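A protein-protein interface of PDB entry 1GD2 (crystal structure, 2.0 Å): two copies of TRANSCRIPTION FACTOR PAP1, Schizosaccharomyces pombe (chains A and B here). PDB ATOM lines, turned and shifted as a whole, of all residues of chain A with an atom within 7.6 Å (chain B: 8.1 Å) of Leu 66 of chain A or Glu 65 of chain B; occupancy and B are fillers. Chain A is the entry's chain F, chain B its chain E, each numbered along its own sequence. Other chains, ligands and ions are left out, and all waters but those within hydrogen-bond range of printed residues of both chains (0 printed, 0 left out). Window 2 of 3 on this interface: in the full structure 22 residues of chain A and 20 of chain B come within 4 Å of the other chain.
Glu 63 of chain B touches Leu 62 of chain A (CG to CD2, 3.5 Å).
CD1 of Leu 62 of chain B touches CG of Glu 63 of chain A (3.4 Å).
Leu 66 of chain B touches Glu 65 of chain A.
CD1 of Leu 66 of chain A touches O of Glu 65 of chain B (3.6 Å).
CD1 of Leu 66 of chain B touches CD1 of Leu 66 of chain A, 3.7 Å away.
Leu 66 of chain A touches just these residues of chain B: Glu 65 (3.6 Å) and Leu 66 (3.7 Å).
Of chain A, only Leu 66 (3.6 Å) comes within 4 Å of Glu 65 of chain B.
Of the printed residues of chain B, Glu 65 of chain A touches Leu 66 (3.2 Å).
Of the printed residues of chain A, Glu 63 of chain B touches Leu 62.
Printed residues of chain B within 4 Å of Leu 62 of chain A: Glu 63 (3.5 Å).
Printed residues of chain A within 4 Å of Leu 62 of chain B: Glu 63 (3.4 Å).
Ile 68 of chain A touches none of the printed residues of chain B.
The nearest residue of chain A that does not touch Glu 65 of chain B is Lys 70 of chain A (7.0 Å).
The nearest printed residue of chain B that does not touch Leu 62 of chain A is Val 59 of chain B (4.01 Å).
Hydrophobic or aromatic side chains of chain A within 4 Å of the printed part of chain B: Leu 62 and Leu 66.
Among the printed residues, no Asp or Glu carboxylate lies within 4 Å of a Lys or Arg side-chain nitrogen of the other chain.
Leu 62 of chain A touches Glu 63 of chain B, and with the chains exchanged Glu 63 of chain A touches Leu 62 of chain B.
Glu 65 of chain A touches Leu 66 of chain B, and with the chains exchanged Leu 66 of chain A touches Glu 65 of chain B.
Leu 66 of chain B touches its own counterpart, Leu 66 of chain A.
Of the 5 pairs that touch across the chains among the printed residues, 5 have their exchanged pair printed and touching as well.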
ATOM      1  N   ARG A  60      -5.531 -12.158  16.089  1.00  0.00           N
ATOM      2  CA  ARG A  60      -6.373 -12.916  17.017  1.00  0.00           C
ATOM      3  C   ARG A  60      -7.680 -13.309  16.317  1.00  0.00           C
ATOM      4  O   ARG A  60      -8.335 -14.282  16.701  1.00  0.00           O
ATOM      5  CB  ARG A  60      -6.666 -12.084  18.268  1.00  0.00           C
ATOM      6  N   GLN A  61      -8.037 -12.542  15.285  1.00  0.00           N
ATOM      7  CA  GLN A  61      -9.242 -12.760  14.481  1.00  0.00           C
ATOM      8  C   GLN A  61      -9.042 -13.911  13.489  1.00  0.00           C
ATOM      9  O   GLN A  61      -9.915 -14.765  13.331  1.00  0.00           O
ATOM     10  CB  GLN A  61      -9.587 -11.472  13.725  1.00  0.00           C
ATOM     11  CG  GLN A  61     -10.720 -11.580  12.709  1.00  0.00           C
ATOM     12  CD  GLN A  61     -10.852 -10.321  11.860  1.00  0.00           C
ATOM     13  OE1 GLN A  61     -10.905  -9.205  12.388  1.00  0.00           O
ATOM     14  NE2 GLN A  61     -10.890 -10.495  10.541  1.00  0.00           N
ATOM     15  N   LEU A  62      -7.893 -13.906  12.817  1.00  0.00           N
ATOM     16  CA  LEU A  62      -7.538 -14.932  11.840  1.00  0.00           C
ATOM     17  C   LEU A  62      -7.157 -16.252  12.497  1.00  0.00           C
ATOM     18  O   LEU A  62      -7.279 -17.310  11.879  1.00  0.00           O
ATOM     19  CB  LEU A  62      -6.384 -14.454  10.957  1.00  0.00           C
ATOM     20  CG  LEU A  62      -6.715 -13.704   9.667  1.00  0.00           C
ATOM     21  CD1 LEU A  62      -7.766 -12.629   9.902  1.00  0.00           C
ATOM     22  CD2 LEU A  62      -5.436 -13.104   9.114  1.00  0.00           C
ATOM     23  N   GLU A  63      -6.667 -16.185  13.733  1.00  0.00           N
ATOM     24  CA  GLU A  63      -6.280 -17.385  14.471  1.00  0.00           C
ATOM     25  C   GLU A  63      -7.492 -18.187  14.940  1.00  0.00           C
ATOM     26  O   GLU A  63      -7.427 -19.415  15.028  1.00  0.00           O
ATOM     27  CB  GLU A  63      -5.375 -17.043  15.656  1.00  0.00           C
ATOM     28  CG  GLU A  63      -3.939 -16.738  15.260  1.00  0.00           C
ATOM     29  CD  GLU A  63      -3.024 -16.539  16.453  1.00  0.00           C
ATOM     30  OE1 GLU A  63      -1.922 -17.125  16.452  1.00  0.00           O
ATOM     31  OE2 GLU A  63      -3.402 -15.796  17.387  1.00  0.00           O
ATOM     32  N   GLU A  64      -8.583 -17.494  15.268  1.00  0.00           N
ATOM     33  CA  GLU A  64      -9.801 -18.177  15.691  1.00  0.00           C
ATOM     34  C   GLU A  64     -10.622 -18.570  14.459  1.00  0.00           C
ATOM     35  O   GLU A  64     -11.391 -19.532  14.504  1.00  0.00           O
ATOM     36  CB  GLU A  64     -10.646 -17.321  16.646  1.00  0.00           C
ATOM     37  CG  GLU A  64     -11.765 -18.135  17.318  1.00  0.00           C
ATOM     38  CD  GLU A  64     -12.628 -17.341  18.292  1.00  0.00           C
ATOM     39  OE1 GLU A  64     -12.110 -16.401  18.935  1.00  0.00           O
ATOM     40  OE2 GLU A  64     -13.829 -17.679  18.429  1.00  0.00           O
ATOM     41  N   GLU A  65     -10.445 -17.834  13.360  1.00  0.00           N
ATOM     42  CA  GLU A  65     -11.157 -18.128  12.121  1.00  0.00           C
ATOM     43  C   GLU A  65     -10.551 -19.368  11.455  1.00  0.00           C
ATOM     44  O   GLU A  65     -11.201 -20.024  10.638  1.00  0.00           O
ATOM     45  CB  GLU A  65     -11.118 -16.933  11.164  1.00  0.00           C
ATOM     46  CG  GLU A  65     -12.093 -17.061   9.999  1.00  0.00           C
ATOM     47  CD  GLU A  65     -11.974 -15.935   8.992  1.00  0.00           C
ATOM     48  OE1 GLU A  65     -11.736 -16.235   7.801  1.00  0.00           O
ATOM     49  OE2 GLU A  65     -12.130 -14.756   9.387  1.00  0.00           O
ATOM     50  N   LEU A  66      -9.293 -19.661  11.779  1.00  0.00           N
ATOM     51  CA  LEU A  66      -8.614 -20.844  11.246  1.00  0.00           C
ATOM     52  C   LEU A  66      -8.915 -22.008  12.199  1.00  0.00           C
ATOM     53  O   LEU A  66      -9.020 -23.160  11.776  1.00  0.00           O
ATOM     54  CB  LEU A  66      -7.097 -20.619  11.149  1.00  0.00           C
ATOM     55  CG  LEU A  66      -6.259 -21.791  10.616  1.00  0.00           C
ATOM     56  CD1 LEU A  66      -6.605 -22.062   9.161  1.00  0.00           C
ATOM     57  CD2 LEU A  66      -4.772 -21.499  10.765  1.00  0.00           C
ATOM     58  N   ARG A  67      -9.072 -21.682  13.481  1.00  0.00           N
ATOM     59  CA  ARG A  67      -9.371 -22.660  14.527  1.00  0.00           C
ATOM     60  C   ARG A  67     -10.766 -23.258  14.291  1.00  0.00           C
ATOM     61  O   ARG A  67     -11.015 -24.435  14.585  1.00  0.00           O
ATOM     62  CB  ARG A  67      -9.290 -21.969  15.904  1.00  0.00           C
ATOM     63  CG  ARG A  67      -9.313 -22.881  17.129  1.00  0.00           C
ATOM     64  CD  ARG A  67     -10.720 -23.069  17.686  1.00  0.00           C
ATOM     65  NE  ARG A  67     -11.290 -21.837  18.233  1.00  0.00           N
ATOM     66  CZ  ARG A  67     -12.545 -21.720  18.664  1.00  0.00           C
ATOM     67  NH1 ARG A  67     -13.370 -22.757  18.614  1.00  0.00           N
ATOM     68  NH2 ARG A  67     -12.976 -20.566  19.159  1.00  0.00           N
ATOM     69  N   ILE A  68     -11.651 -22.447  13.717  1.00  0.00           N
ATOM     70  CA  ILE A  68     -13.021 -22.850  13.425  1.00  0.00           C
ATOM     71  C   ILE A  68     -13.149 -23.624  12.105  1.00  0.00           C
ATOM     72  O   ILE A  68     -13.676 -24.736  12.086  1.00  0.00           O
ATOM     73  CB  ILE A  68     -13.965 -21.610  13.442  1.00  0.00           C
ATOM     74  CG1 ILE A  68     -14.058 -21.054  14.868  1.00  0.00           C
ATOM     75  CG2 ILE A  68     -15.350 -21.966  12.926  1.00  0.00           C
ATOM     76  CD1 ILE A  68     -14.827 -19.754  14.989  1.00  0.00           C
ATOM     77  N   LEU A  69     -12.627 -23.055  11.021  1.00  0.00           N
ATOM     78  CA  LEU A  69     -12.698 -23.678   9.697  1.00  0.00           C
ATOM     79  C   LEU A  69     -11.791 -24.882   9.459  1.00  0.00           C
ATOM     80  O   LEU A  69     -11.818 -25.479   8.378  1.00  0.00           O
ATOM     81  CB  LEU A  69     -12.462 -22.633   8.606  1.00  0.00           C
ATOM     82  CG  LEU A  69     -13.692 -21.890   8.078  1.00  0.00           C
ATOM     83  CD1 LEU A  69     -14.534 -21.316   9.210  1.00  0.00           C
ATOM     84  CD2 LEU A  69     -13.225 -20.798   7.132  1.00  0.00           C
ATOM     85  N   LYS A  70     -10.974 -25.222  10.454  1.00  0.00           N
ATOM     86  CA  LYS A  70     -10.073 -26.370  10.353  1.00  0.00           C
ATOM     87  C   LYS A  70     -10.535 -27.457  11.321  1.00  0.00           C
ATOM     88  O   LYS A  70     -10.204 -27.350  12.523  1.00  0.00           O
ATOM     89  CB  LYS A  70      -8.628 -25.958  10.656  1.00  0.00           C
ATOM     90  OXT LYS A  70     -11.250 -28.383  10.870  1.00  0.00           O
ATOM     91  N   VAL B  59       0.377 -11.991   9.659  1.00  0.00           N
ATOM     92  CA  VAL B  59      -0.941 -11.720   9.093  1.00  0.00           C
ATOM     93  C   VAL B  59      -0.993 -12.206   7.637  1.00  0.00           C
ATOM     94  O   VAL B  59      -2.036 -12.125   6.989  1.00  0.00           O
ATOM     95  CB  VAL B  59      -1.327 -10.212   9.191  1.00  0.00           C
ATOM     96  CG1 VAL B  59      -0.642  -9.396   8.100  1.00  0.00           C
ATOM     97  CG2 VAL B  59      -2.838 -10.045   9.132  1.00  0.00           C
ATOM     98  N   ARG B  60       0.139 -12.685   7.121  1.00  0.00           N
ATOM     99  CA  ARG B  60       0.204 -13.212   5.756  1.00  0.00           C
ATOM    100  C   ARG B  60       0.400 -14.733   5.805  1.00  0.00           C
ATOM    101  O   ARG B  60       0.032 -15.446   4.867  1.00  0.00           O
ATOM    102  CB  ARG B  60       1.314 -12.537   4.931  1.00  0.00           C
ATOM    103  CG  ARG B  60       2.731 -13.060   5.167  1.00  0.00           C
ATOM    104  CD  ARG B  60       3.726 -12.427   4.199  1.00  0.00           C
ATOM    105  NE  ARG B  60       3.759 -10.971   4.328  1.00  0.00           N
ATOM    106  CZ  ARG B  60       4.777 -10.280   4.834  1.00  0.00           C
ATOM    107  NH1 ARG B  60       5.869 -10.906   5.261  1.00  0.00           N
ATOM    108  NH2 ARG B  60       4.690  -8.959   4.942  1.00  0.00           N
ATOM    109  N   GLN B  61       0.989 -15.218   6.900  1.00  0.00           N
ATOM    110  CA  GLN B  61       1.211 -16.649   7.105  1.00  0.00           C
ATOM    111  C   GLN B  61      -0.128 -17.302   7.440  1.00  0.00           C
ATOM    112  O   GLN B  61      -0.387 -18.445   7.055  1.00  0.00           O
ATOM    113  CB  GLN B  61       2.187 -16.895   8.262  1.00  0.00           C
ATOM    114  CG  GLN B  61       3.636 -16.524   7.982  1.00  0.00           C
ATOM    115  CD  GLN B  61       4.569 -16.888   9.132  1.00  0.00           C
ATOM    116  OE1 GLN B  61       4.125 -17.155  10.254  1.00  0.00           O
ATOM    117  NE2 GLN B  61       5.870 -16.906   8.853  1.00  0.00           N
ATOM    118  N   LEU B  62      -0.965 -16.562   8.171  1.00  0.00           N
ATOM    119  CA  LEU B  62      -2.289 -17.026   8.578  1.00  0.00           C
ATOM    120  C   LEU B  62      -3.347 -16.831   7.492  1.00  0.00           C
ATOM    121  O   LEU B  62      -4.429 -17.415   7.568  1.00  0.00           O
ATOM    122  CB  LEU B  62      -2.731 -16.330   9.865  1.00  0.00           C
ATOM    123  CG  LEU B  62      -1.890 -16.585  11.115  1.00  0.00           C
ATOM    124  CD1 LEU B  62      -2.498 -15.832  12.281  1.00  0.00           C
ATOM    125  CD2 LEU B  62      -1.806 -18.075  11.421  1.00  0.00           C
ATOM    126  N   GLU B  63      -3.053 -15.978   6.511  1.00  0.00           N
ATOM    127  CA  GLU B  63      -3.975 -15.739   5.401  1.00  0.00           C
ATOM    128  C   GLU B  63      -3.726 -16.735   4.267  1.00  0.00           C
ATOM    129  O   GLU B  63      -4.587 -16.934   3.405  1.00  0.00           O
ATOM    130  CB  GLU B  63      -3.871 -14.301   4.881  1.00  0.00           C
ATOM    131  CG  GLU B  63      -4.650 -13.287   5.716  1.00  0.00           C
ATOM    132  CD  GLU B  63      -4.665 -11.887   5.116  1.00  0.00           C
ATOM    133  OE1 GLU B  63      -3.779 -11.571   4.287  1.00  0.00           O
ATOM    134  OE2 GLU B  63      -5.567 -11.098   5.483  1.00  0.00           O
ATOM    135  N   GLU B  64      -2.536 -17.340   4.266  1.00  0.00           N
ATOM    136  CA  GLU B  64      -2.166 -18.341   3.268  1.00  0.00           C
ATOM    137  C   GLU B  64      -2.618 -19.707   3.786  1.00  0.00           C
ATOM    138  O   GLU B  64      -2.923 -20.616   3.012  1.00  0.00           O
ATOM    139  CB  GLU B  64      -0.652 -18.330   3.043  1.00  0.00           C
ATOM    140  CG  GLU B  64      -0.163 -19.289   1.960  1.00  0.00           C
ATOM    141  CD  GLU B  64      -0.759 -18.999   0.587  1.00  0.00           C
ATOM    142  OE1 GLU B  64      -1.269 -19.950  -0.048  1.00  0.00           O
ATOM    143  OE2 GLU B  64      -0.714 -17.829   0.140  1.00  0.00           O
ATOM    144  N   GLU B  65      -2.672 -19.826   5.111  1.00  0.00           N
ATOM    145  CA  GLU B  65      -3.094 -21.049   5.783  1.00  0.00           C
ATOM    146  C   GLU B  65      -4.626 -21.153   5.799  1.00  0.00           C
ATOM    147  O   GLU B  65      -5.183 -22.253   5.866  1.00  0.00           O
ATOM    148  CB  GLU B  65      -2.544 -21.075   7.217  1.00  0.00           C
ATOM    149  CG  GLU B  65      -2.586 -22.444   7.883  1.00  0.00           C
ATOM    150  CD  GLU B  65      -1.875 -23.516   7.060  1.00  0.00           C
ATOM    151  OE1 GLU B  65      -0.656 -23.370   6.811  1.00  0.00           O
ATOM    152  OE2 GLU B  65      -2.542 -24.497   6.653  1.00  0.00           O
ATOM    153  N   LEU B  66      -5.292 -20.001   5.731  1.00  0.00           N
ATOM    154  CA  LEU B  66      -6.754 -19.931   5.733  1.00  0.00           C
ATOM    155  C   LEU B  66      -7.285 -19.707   4.312  1.00  0.00           C
ATOM    156  O   LEU B  66      -8.444 -19.327   4.123  1.00  0.00           O
ATOM    157  CB  LEU B  66      -7.225 -18.812   6.677  1.00  0.00           C
ATOM    158  CG  LEU B  66      -8.703 -18.642   7.051  1.00  0.00           C
ATOM    159  CD1 LEU B  66      -9.260 -19.904   7.682  1.00  0.00           C
ATOM    160  CD2 LEU B  66      -8.829 -17.484   8.012  1.00  0.00           C
ATOM    161  N   ARG B  67      -6.425 -19.937   3.319  1.00  0.00           N
ATOM    162  CA  ARG B  67      -6.796 -19.784   1.912  1.00  0.00           C
ATOM    163  C   ARG B  67      -6.788 -21.140   1.206  1.00  0.00           C
ATOM    164  O   ARG B  67      -7.409 -21.304   0.152  1.00  0.00           O
ATOM    165  CB  ARG B  67      -5.847 -18.818   1.209  1.00  0.00           C
ATOM    166  N   ILE B  68      -6.082 -22.103   1.798  1.00  0.00           N
ATOM    167  CA  ILE B  68      -5.978 -23.457   1.251  1.00  0.00           C
ATOM    168  C   ILE B  68      -6.963 -24.454   1.893  1.00  0.00           C
ATOM    169  O   ILE B  68      -7.435 -25.386   1.231  1.00  0.00           O
ATOM    170  CB  ILE B  68      -4.510 -23.995   1.338  1.00  0.00           C
ATOM    171  CG1 ILE B  68      -3.949 -23.834   2.757  1.00  0.00           C
ATOM    172  CG2 ILE B  68      -3.623 -23.263   0.335  1.00  0.00           C
ATOM    173  CD1 ILE B  68      -2.509 -24.304   2.916  1.00  0.00           C
ATOM    174  N   LEU B  69      -7.290 -24.234   3.166  1.00  0.00           N
ATOM    175  CA  LEU B  69      -8.220 -25.096   3.897  1.00  0.00           C
ATOM    176  C   LEU B  69      -8.741 -24.416   5.174  1.00  0.00           C
ATOM    177  O   LEU B  69      -9.596 -23.513   5.038  1.00  0.00           O
ATOM    178  CB  LEU B  69      -7.554 -26.441   4.224  1.00  0.00           C
